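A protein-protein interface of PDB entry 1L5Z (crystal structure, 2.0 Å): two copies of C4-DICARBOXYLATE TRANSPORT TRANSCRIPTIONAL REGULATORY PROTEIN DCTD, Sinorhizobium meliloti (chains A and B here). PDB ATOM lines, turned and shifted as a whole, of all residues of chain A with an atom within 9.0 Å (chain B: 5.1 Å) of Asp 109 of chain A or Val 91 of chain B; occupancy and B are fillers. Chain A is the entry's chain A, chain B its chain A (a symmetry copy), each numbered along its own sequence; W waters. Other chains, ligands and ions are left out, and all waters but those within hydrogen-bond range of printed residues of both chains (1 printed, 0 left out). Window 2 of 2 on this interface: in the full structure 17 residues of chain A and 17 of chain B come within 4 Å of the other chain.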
ATOM      1  N   THR A  22     -30.463   2.519   1.754  1.00  0.00           N
ATOM      2  CA  THR A  22     -29.239   3.343   1.621  1.00  0.00           C
ATOM      3  C   THR A  22     -29.267   4.522   2.590  1.00  0.00           C
ATOM      4  O   THR A  22     -28.284   4.803   3.305  1.00  0.00           O
ATOM      5  CB  THR A  22     -29.071   3.920   0.195  1.00  0.00           C
ATOM      6  OG1 THR A  22     -29.056   2.850  -0.748  1.00  0.00           O
ATOM      7  CG2 THR A  22     -27.733   4.729   0.089  1.00  0.00           C
ATOM      8  N   LEU A  23     -30.409   5.198   2.623  1.00  0.00           N
ATOM      9  CA  LEU A  23     -30.598   6.362   3.478  1.00  0.00           C
ATOM     10  C   LEU A  23     -30.596   5.985   4.971  1.00  0.00           C
ATOM     11  O   LEU A  23     -29.945   6.640   5.795  1.00  0.00           O
ATOM     12  CB  LEU A  23     -31.921   7.040   3.104  1.00  0.00           C
ATOM     13  CG  LEU A  23     -31.941   7.766   1.725  1.00  0.00           C
ATOM     14  CD1 LEU A  23     -33.364   8.155   1.350  1.00  0.00           C
ATOM     15  CD2 LEU A  23     -31.088   9.012   1.800  1.00  0.00           C
ATOM     16  N   ALA A  26     -27.461   5.328   6.291  1.00  0.00           N
ATOM     17  CA  ALA A  26     -26.681   6.571   6.373  1.00  0.00           C
ATOM     18  C   ALA A  26     -27.144   7.424   7.582  1.00  0.00           C
ATOM     19  O   ALA A  26     -26.694   8.550   7.761  1.00  0.00           O
ATOM     20  CB  ALA A  26     -26.796   7.397   5.048  1.00  0.00           C
ATOM     21  N   PHE A  28     -30.467   8.263   8.314  1.00  0.00           N
ATOM     22  CA  PHE A  28     -31.749   8.950   8.170  1.00  0.00           C
ATOM     23  C   PHE A  28     -32.930   8.099   8.669  1.00  0.00           C
ATOM     24  O   PHE A  28     -32.886   6.870   8.611  1.00  0.00           O
ATOM     25  CB  PHE A  28     -32.073   9.268   6.686  1.00  0.00           C
ATOM     26  CG  PHE A  28     -31.168  10.286   6.049  1.00  0.00           C
ATOM     27  CD1 PHE A  28     -29.933   9.924   5.536  1.00  0.00           C
ATOM     28  CD2 PHE A  28     -31.544  11.627   6.005  1.00  0.00           C
ATOM     29  CE1 PHE A  28     -29.062  10.886   4.982  1.00  0.00           C
ATOM     30  CE2 PHE A  28     -30.701  12.587   5.466  1.00  0.00           C
ATOM     31  CZ  PHE A  28     -29.457  12.229   4.952  1.00  0.00           C
ATOM     32  N   ILE A 102     -30.781  13.449  -8.798  1.00  0.00           N
ATOM     33  CA  ILE A 102     -29.903  12.287  -8.726  1.00  0.00           C
ATOM     34  C   ILE A 102     -30.231  11.499  -9.986  1.00  0.00           C
ATOM     35  O   ILE A 102     -31.415  11.324 -10.289  1.00  0.00           O
ATOM     36  CB  ILE A 102     -30.294  11.446  -7.502  1.00  0.00           C
ATOM     37  CG1 ILE A 102     -29.804  12.165  -6.257  1.00  0.00           C
ATOM     38  CG2 ILE A 102     -29.686  10.054  -7.571  1.00  0.00           C
ATOM     39  CD1 ILE A 102     -28.312  12.356  -6.323  1.00  0.00           C
ATOM     40  N   PRO A 105     -29.329   4.723 -13.098  1.00  0.00           N
ATOM     41  CA  PRO A 105     -29.634   3.959 -11.880  1.00  0.00           C
ATOM     42  C   PRO A 105     -28.899   4.677 -10.736  1.00  0.00           C
ATOM     43  O   PRO A 105     -27.758   5.117 -10.903  1.00  0.00           O
ATOM     44  CB  PRO A 105     -29.089   2.552 -12.195  1.00  0.00           C
ATOM     45  CG  PRO A 105     -27.965   2.830 -13.171  1.00  0.00           C
ATOM     46  CD  PRO A 105     -28.562   3.924 -14.069  1.00  0.00           C
ATOM     47  N   PHE A 106     -29.526   4.778  -9.570  1.00  0.00           N
ATOM     48  CA  PHE A 106     -28.898   5.576  -8.528  1.00  0.00           C
ATOM     49  C   PHE A 106     -27.614   5.012  -7.955  1.00  0.00           C
ATOM     50  O   PHE A 106     -27.457   3.811  -7.817  1.00  0.00           O
ATOM     51  CB  PHE A 106     -29.928   5.888  -7.421  1.00  0.00           C
ATOM     52  CG  PHE A 106     -30.061   4.800  -6.368  1.00  0.00           C
ATOM     53  CD1 PHE A 106     -30.876   3.714  -6.585  1.00  0.00           C
ATOM     54  CD2 PHE A 106     -29.343   4.873  -5.177  1.00  0.00           C
ATOM     55  CE1 PHE A 106     -30.988   2.684  -5.626  1.00  0.00           C
ATOM     56  CE2 PHE A 106     -29.434   3.857  -4.201  1.00  0.00           C
ATOM     57  CZ  PHE A 106     -30.261   2.760  -4.435  1.00  0.00           C
ATOM     58  N   ALA A 107     -26.660   5.894  -7.691  1.00  0.00           N
ATOM     59  CA  ALA A 107     -25.396   5.493  -7.058  1.00  0.00           C
ATOM     60  C   ALA A 107     -25.674   5.771  -5.578  1.00  0.00           C
ATOM     61  O   ALA A 107     -26.099   6.875  -5.223  1.00  0.00           O
ATOM     62  CB  ALA A 107     -24.250   6.366  -7.558  1.00  0.00           C
ATOM     63  N   ALA A 108     -25.461   4.773  -4.728  1.00  0.00           N
ATOM     64  CA  ALA A 108     -25.723   4.901  -3.311  1.00  0.00           C
ATOM     65  C   ALA A 108     -25.003   6.098  -2.666  1.00  0.00           C
ATOM     66  O   ALA A 108     -25.607   6.853  -1.886  1.00  0.00           O
ATOM     67  CB  ALA A 108     -25.323   3.579  -2.583  1.00  0.00           C
ATOM     68  N   ASP A 109     -23.722   6.267  -2.973  1.00  0.00           N
ATOM     69  CA  ASP A 109     -23.012   7.379  -2.371  1.00  0.00           C
ATOM     70  C   ASP A 109     -23.515   8.744  -2.799  1.00  0.00           C
ATOM     71  O   ASP A 109     -23.561   9.669  -1.965  1.00  0.00           O
ATOM     72  CB  ASP A 109     -21.498   7.280  -2.605  1.00  0.00           C
ATOM     73  CG  ASP A 109     -21.097   7.213  -4.082  1.00  0.00           C
ATOM     74  OD1 ASP A 109     -21.912   7.298  -5.025  1.00  0.00           O
ATOM     75  OD2 ASP A 109     -19.887   7.060  -4.295  1.00  0.00           O
ATOM     76  N   ARG A 110     -23.897   8.885  -4.068  1.00  0.00           N
ATOM     77  CA  ARG A 110     -24.376  10.185  -4.552  1.00  0.00           C
ATOM     78  C   ARG A 110     -25.723  10.499  -3.873  1.00  0.00           C
ATOM     79  O   ARG A 110     -26.011  11.650  -3.500  1.00  0.00           O
ATOM     80  CB  ARG A 110     -24.564  10.148  -6.070  1.00  0.00           C
ATOM     81  CG  ARG A 110     -23.305   9.775  -6.843  1.00  0.00           C
ATOM     82  CD  ARG A 110     -22.324  10.917  -6.858  1.00  0.00           C
ATOM     83  NE  ARG A 110     -22.324  11.532  -8.188  1.00  0.00           N
ATOM     84  CZ  ARG A 110     -21.625  11.093  -9.238  1.00  0.00           C
ATOM     85  NH1 ARG A 110     -20.820  10.038  -9.156  1.00  0.00           N
ATOM     86  NH2 ARG A 110     -21.788  11.682 -10.400  1.00  0.00           N
ATOM     87  N   LEU A 111     -26.535   9.467  -3.715  1.00  0.00           N
ATOM     88  CA  LEU A 111     -27.844   9.638  -3.074  1.00  0.00           C
ATOM     89  C   LEU A 111     -27.623  10.153  -1.637  1.00  0.00           C
ATOM     90  O   LEU A 111     -28.290  11.079  -1.166  1.00  0.00           O
ATOM     91  CB  LEU A 111     -28.598   8.303  -3.003  1.00  0.00           C
ATOM     92  CG  LEU A 111     -29.866   8.291  -2.102  1.00  0.00           C
ATOM     93  CD1 LEU A 111     -30.885   9.293  -2.613  1.00  0.00           C
ATOM     94  CD2 LEU A 111     -30.545   6.899  -2.157  1.00  0.00           C
ATOM     95  N   VAL A 112     -26.694   9.531  -0.933  1.00  0.00           N
ATOM     96  CA  VAL A 112     -26.448   9.933   0.451  1.00  0.00           C
ATOM     97  C   VAL A 112     -25.907  11.382   0.521  1.00  0.00           C
ATOM     98  O   VAL A 112     -26.350  12.178   1.351  1.00  0.00           O
ATOM     99  CB  VAL A 112     -25.449   8.955   1.133  1.00  0.00           C
ATOM    100  CG1 VAL A 112     -24.944   9.563   2.456  1.00  0.00           C
ATOM    101  CG2 VAL A 112     -26.173   7.533   1.401  1.00  0.00           C
ATOM    102  N   GLN A 113     -24.968  11.721  -0.355  1.00  0.00           N
ATOM    103  CA  GLN A 113     -24.424  13.076  -0.337  1.00  0.00           C
ATOM    104  C   GLN A 113     -25.491  14.132  -0.643  1.00  0.00           C
ATOM    105  O   GLN A 113     -25.582  15.157   0.030  1.00  0.00           O
ATOM    106  CB  GLN A 113     -23.242  13.192  -1.331  1.00  0.00           C
ATOM    107  CG  GLN A 113     -22.080  12.324  -0.893  1.00  0.00           C
ATOM    108  CD  GLN A 113     -20.853  12.451  -1.768  1.00  0.00           C
ATOM    109  OE1 GLN A 113     -20.873  13.055  -2.864  1.00  0.00           O
ATOM    110  NE2 GLN A 113     -19.762  11.860  -1.293  1.00  0.00           N
ATOM    111  N   SER A 114     -26.299  13.866  -1.659  1.00  0.00           N
ATOM    112  CA  SER A 114     -27.350  14.804  -2.045  1.00  0.00           C
ATOM    113  C   SER A 114     -28.353  14.961  -0.878  1.00  0.00           C
ATOM    114  O   SER A 114     -28.738  16.077  -0.524  1.00  0.00           O
ATOM    115  CB  SER A 114     -28.039  14.290  -3.326  1.00  0.00           C
ATOM    116  OG  SER A 114     -29.123  15.092  -3.713  1.00  0.00           O
ATOM    117  N   ALA A 115     -28.745  13.852  -0.253  1.00  0.00           N
ATOM    118  CA  ALA A 115     -29.701  13.928   0.881  1.00  0.00           C
ATOM    119  C   ALA A 115     -29.107  14.693   2.076  1.00  0.00           C
ATOM    120  O   ALA A 115     -29.790  15.443   2.760  1.00  0.00           O
ATOM    121  CB  ALA A 115     -30.115  12.455   1.341  1.00  0.00           C
ATOM    122  N   ARG A 116     -27.833  14.462   2.354  1.00  0.00           N
ATOM    123  CA  ARG A 116     -27.187  15.137   3.478  1.00  0.00           C
ATOM    124  C   ARG A 116     -27.090  16.635   3.246  1.00  0.00           C
ATOM    125  O   ARG A 116     -27.308  17.422   4.170  1.00  0.00           O
ATOM    126  CB  ARG A 116     -25.800  14.530   3.757  1.00  0.00           C
ATOM    127  CG  ARG A 116     -25.916  13.202   4.586  1.00  0.00           C
ATOM    128  CD  ARG A 116     -24.554  12.492   4.794  1.00  0.00           C
ATOM    129  NE  ARG A 116     -24.727  11.404   5.760  1.00  0.00           N
ATOM    130  CZ  ARG A 116     -23.850  10.425   5.944  1.00  0.00           C
ATOM    131  NH1 ARG A 116     -22.750  10.419   5.217  1.00  0.00           N
ATOM    132  NH2 ARG A 116     -24.079   9.464   6.844  1.00  0.00           N
ATOM    133  N   ARG A 117     -26.801  17.039   2.011  1.00  0.00           N
ATOM    134  CA  ARG A 117     -26.709  18.476   1.718  1.00  0.00           C
ATOM    135  C   ARG A 117     -28.091  19.123   1.870  1.00  0.00           C
ATOM    136  O   ARG A 117     -28.215  20.182   2.483  1.00  0.00           O
ATOM    137  CB  ARG A 117     -26.180  18.691   0.292  1.00  0.00           C
ATOM    138  CG  ARG A 117     -25.963  20.153  -0.101  1.00  0.00           C
ATOM    139  CD  ARG A 117     -25.029  20.237  -1.360  1.00  0.00           C
ATOM    140  NE  ARG A 117     -25.537  19.395  -2.430  1.00  0.00           N
ATOM    141  CZ  ARG A 117     -24.830  18.490  -3.105  1.00  0.00           C
ATOM    142  NH1 ARG A 117     -23.546  18.284  -2.852  1.00  0.00           N
ATOM    143  NH2 ARG A 117     -25.445  17.740  -4.014  1.00  0.00           N
ATOM    144  N   ILE B  87     -13.647  12.753 -11.120  1.00  0.00           N
ATOM    145  CA  ILE B  87     -14.916  12.749 -10.390  1.00  0.00           C
ATOM    146  C   ILE B  87     -14.899  11.873  -9.110  1.00  0.00           C
ATOM    147  O   ILE B  87     -15.317  12.323  -8.047  1.00  0.00           O
ATOM    148  CB  ILE B  87     -16.091  12.377 -11.340  1.00  0.00           C
ATOM    149  CG1 ILE B  87     -16.402  13.595 -12.212  1.00  0.00           C
ATOM    150  CG2 ILE B  87     -17.359  11.999 -10.547  1.00  0.00           C
ATOM    151  CD1 ILE B  87     -17.437  13.348 -13.300  1.00  0.00           C
ATOM    152  N   PRO B  88     -14.371  10.631  -9.183  1.00  0.00           N
ATOM    153  CA  PRO B  88     -14.366   9.813  -7.958  1.00  0.00           C
ATOM    154  C   PRO B  88     -13.686  10.507  -6.777  1.00  0.00           C
ATOM    155  O   PRO B  88     -14.129  10.405  -5.646  1.00  0.00           O
ATOM    156  CB  PRO B  88     -13.617   8.542  -8.379  1.00  0.00           C
ATOM    157  CG  PRO B  88     -13.955   8.434  -9.867  1.00  0.00           C
ATOM    158  CD  PRO B  88     -13.851   9.873 -10.342  1.00  0.00           C
ATOM    159  N   MET B  89     -12.594  11.210  -7.052  1.00  0.00           N
ATOM    160  CA  MET B  89     -11.879  11.921  -6.006  1.00  0.00           C
ATOM    161  C   MET B  89     -12.708  13.068  -5.435  1.00  0.00           C
ATOM    162  O   MET B  89     -12.673  13.327  -4.229  1.00  0.00           O
ATOM    163  CB  MET B  89     -10.594  12.523  -6.549  1.00  0.00           C
ATOM    164  CG  MET B  89      -9.439  12.236  -5.687  1.00  0.00           C
ATOM    165  SD  MET B  89      -7.981  13.157  -6.230  1.00  0.00           S
ATOM    166  CE  MET B  89      -7.622  12.444  -7.835  1.00  0.00           C
ATOM    167  N   ALA B  90     -13.376  13.784  -6.338  1.00  0.00           N
ATOM    168  CA  ALA B  90     -14.221  14.913  -5.961  1.00  0.00           C
ATOM    169  C   ALA B  90     -15.361  14.380  -5.087  1.00  0.00           C
ATOM    170  O   ALA B  90     -15.742  15.025  -4.134  1.00  0.00           O
ATOM    171  CB  ALA B  90     -14.763  15.597  -7.209  1.00  0.00           C
ATOM    172  N   VAL B  91     -15.901  13.206  -5.420  1.00  0.00           N
ATOM    173  CA  VAL B  91     -16.973  12.596  -4.613  1.00  0.00           C
ATOM    174  C   VAL B  91     -16.387  12.232  -3.255  1.00  0.00           C
ATOM    175  O   VAL B  91     -17.007  12.467  -2.217  1.00  0.00           O
ATOM    176  CB  VAL B  91     -17.570  11.363  -5.332  1.00  0.00           C
ATOM    177  CG1 VAL B  91     -18.532  10.559  -4.399  1.00  0.00           C
ATOM    178  CG2 VAL B  91     -18.349  11.867  -6.550  1.00  0.00           C
ATOM    179  N   GLN B  92     -15.164  11.696  -3.243  1.00  0.00           N
ATOM    180  CA  GLN B  92     -14.536  11.417  -1.965  1.00  0.00           C
ATOM    181  C   GLN B  92     -14.349  12.718  -1.177  1.00  0.00           C
ATOM    182  O   GLN B  92     -14.498  12.740   0.053  1.00  0.00           O
ATOM    183  CB  GLN B  92     -13.161  10.769  -2.162  1.00  0.00           C
ATOM    184  CG  GLN B  92     -12.410  10.596  -0.853  1.00  0.00           C
ATOM    185  CD  GLN B  92     -13.060   9.549   0.061  1.00  0.00           C
ATOM    186  OE1 GLN B  92     -13.288   8.417  -0.351  1.00  0.00           O
ATOM    187  NE2 GLN B  92     -13.361   9.931   1.286  1.00  0.00           N
ATOM    188  N   ALA B  93     -13.985  13.807  -1.874  1.00  0.00           N
ATOM    189  CA  ALA B  93     -13.756  15.059  -1.176  1.00  0.00           C
ATOM    190  C   ALA B  93     -15.064  15.543  -0.558  1.00  0.00           C
ATOM    191  O   ALA B  93     -15.070  16.107   0.542  1.00  0.00           O
ATOM    192  CB  ALA B  93     -13.173  16.142  -2.132  1.00  0.00           C
ATOM    193  N   ILE B  94     -16.172  15.340  -1.275  1.00  0.00           N
ATOM    194  CA  ILE B  94     -17.466  15.770  -0.747  1.00  0.00           C
ATOM    195  C   ILE B  94     -17.753  14.967   0.534  1.00  0.00           C
ATOM    196  O   ILE B  94     -18.156  15.528   1.543  1.00  0.00           O
ATOM    197  CB  ILE B  94     -18.599  15.622  -1.827  1.00  0.00           C
ATOM    198  CG1 ILE B  94     -18.366  16.657  -2.953  1.00  0.00           C
ATOM    199  CG2 ILE B  94     -20.028  15.891  -1.182  1.00  0.00           C
ATOM    200  CD1 ILE B  94     -19.386  16.534  -4.092  1.00  0.00           C
ATOM    201  N   GLN B  95     -17.482  13.661   0.506  1.00  0.00           N
ATOM    202  CA  GLN B  95     -17.680  12.842   1.700  1.00  0.00           C
ATOM    203  C   GLN B  95     -16.851  13.455   2.826  1.00  0.00           C
ATOM    204  O   GLN B  95     -17.241  13.389   3.987  1.00  0.00           O
ATOM    205  CB  GLN B  95     -17.217  11.409   1.453  1.00  0.00           C
ATOM    206  CG  GLN B  95     -17.393  10.460   2.643  1.00  0.00           C
ATOM    207  CD  GLN B  95     -16.984   9.034   2.294  1.00  0.00           C
ATOM    208  OE1 GLN B  95     -16.031   8.482   2.875  1.00  0.00           O
ATOM    209  NE2 GLN B  95     -17.694   8.430   1.333  1.00  0.00           N
ATOM    210  N   PHE B 101     -19.481  19.414  -6.630  1.00  0.00           N
ATOM    211  CA  PHE B 101     -18.557  19.429  -7.774  1.00  0.00           C
ATOM    212  C   PHE B 101     -19.355  19.695  -9.043  1.00  0.00           C
ATOM    213  O   PHE B 101     -20.571  19.460  -9.102  1.00  0.00           O
ATOM    214  CB  PHE B 101     -17.733  18.117  -7.934  1.00  0.00           C
ATOM    215  CG  PHE B 101     -18.474  16.991  -8.584  1.00  0.00           C
ATOM    216  CD1 PHE B 101     -18.575  16.908  -9.971  1.00  0.00           C
ATOM    217  CD2 PHE B 101     -19.090  16.013  -7.804  1.00  0.00           C
ATOM    218  CE1 PHE B 101     -19.282  15.863 -10.592  1.00  0.00           C
ATOM    219  CE2 PHE B 101     -19.806  14.954  -8.401  1.00  0.00           C
ATOM    220  CZ  PHE B 101     -19.903  14.877  -9.804  1.00  0.00           C
HETATM  221  O   HOH W   1     -20.877   9.496   0.568  1.00  0.00           O
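The side-chain amide oxygen (OE1) of Gln 95 of chain B lies within hydrogen-bond range of the side-chain amide nitrogen (NE2) of Gln 92 of chain B, at 3.4 Å.
No position is printed for both chains.
NE2 of Gln 113 of chain A sits at hydrogen-bond distance from O of Val 91 of chain B (3.0 Å).
NE2 of Gln 113 of chain A sits close to N of Gln 95 of chain B, at 3.4 Å.
Water W1 bridges NE2 of Gln 113 of chain A (3.2 Å) and NE2 of Gln 95 of chain B (3.4 Å).
Of the 10 printed residues of chain B, 4 touch a printed residue of chain A.
Hydrophobic or aromatic side chains of chain B within 4 Å of the printed part of chain A: Val 91, Ile 94 and Phe 101.
Printed residues of chain A that touch a printed residue of chain B: Asp 109, Arg 110 and Gln 113.
Among the printed residues, no Asp or Glu carboxylate lies within 4 Å of a Lys or Arg side-chain nitrogen of the other chain.
Among the printed residues, pairs that only touch across the chains: Asp 109 of chain A with Val 91 of chain B, Arg 110 of chain A with Phe 101 of chain B and Gln 113 of chain A with Ile 94 of chain B.
Phe 28 of chain A touches none of the printed residues of chain B.
Of chain B, only Val 91 comes within 4 Å of Asp 109 of chain A.
Of the printed residues of chain B, Arg 110 of chain A touches Phe 101 (3.8 Å).
Printed residues of chain B within 4 Å of Gln 113 of chain A: Val 91 (3.0 Å), Ile 94 (3.4 Å) and Gln 95 (3.4 Å).
Of the printed residues of chain A, Ile 94 of chain B touches Gln 113.
Of the printed residues of chain A, Gln 95 of chain B touches Gln 113 (3.4 Å).
Printed residues of chain A within 4 Å of Phe 101 of chain B: Arg 110 (3.8 Å).
The nearest printed residue of chain B that does not touch Asp 109 of chain A is Gln 95 of chain B (5.6 Å).
The nearest residue of chain A that does not touch Val 91 of chain B is Arg 110 of chain A (4.03 Å).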
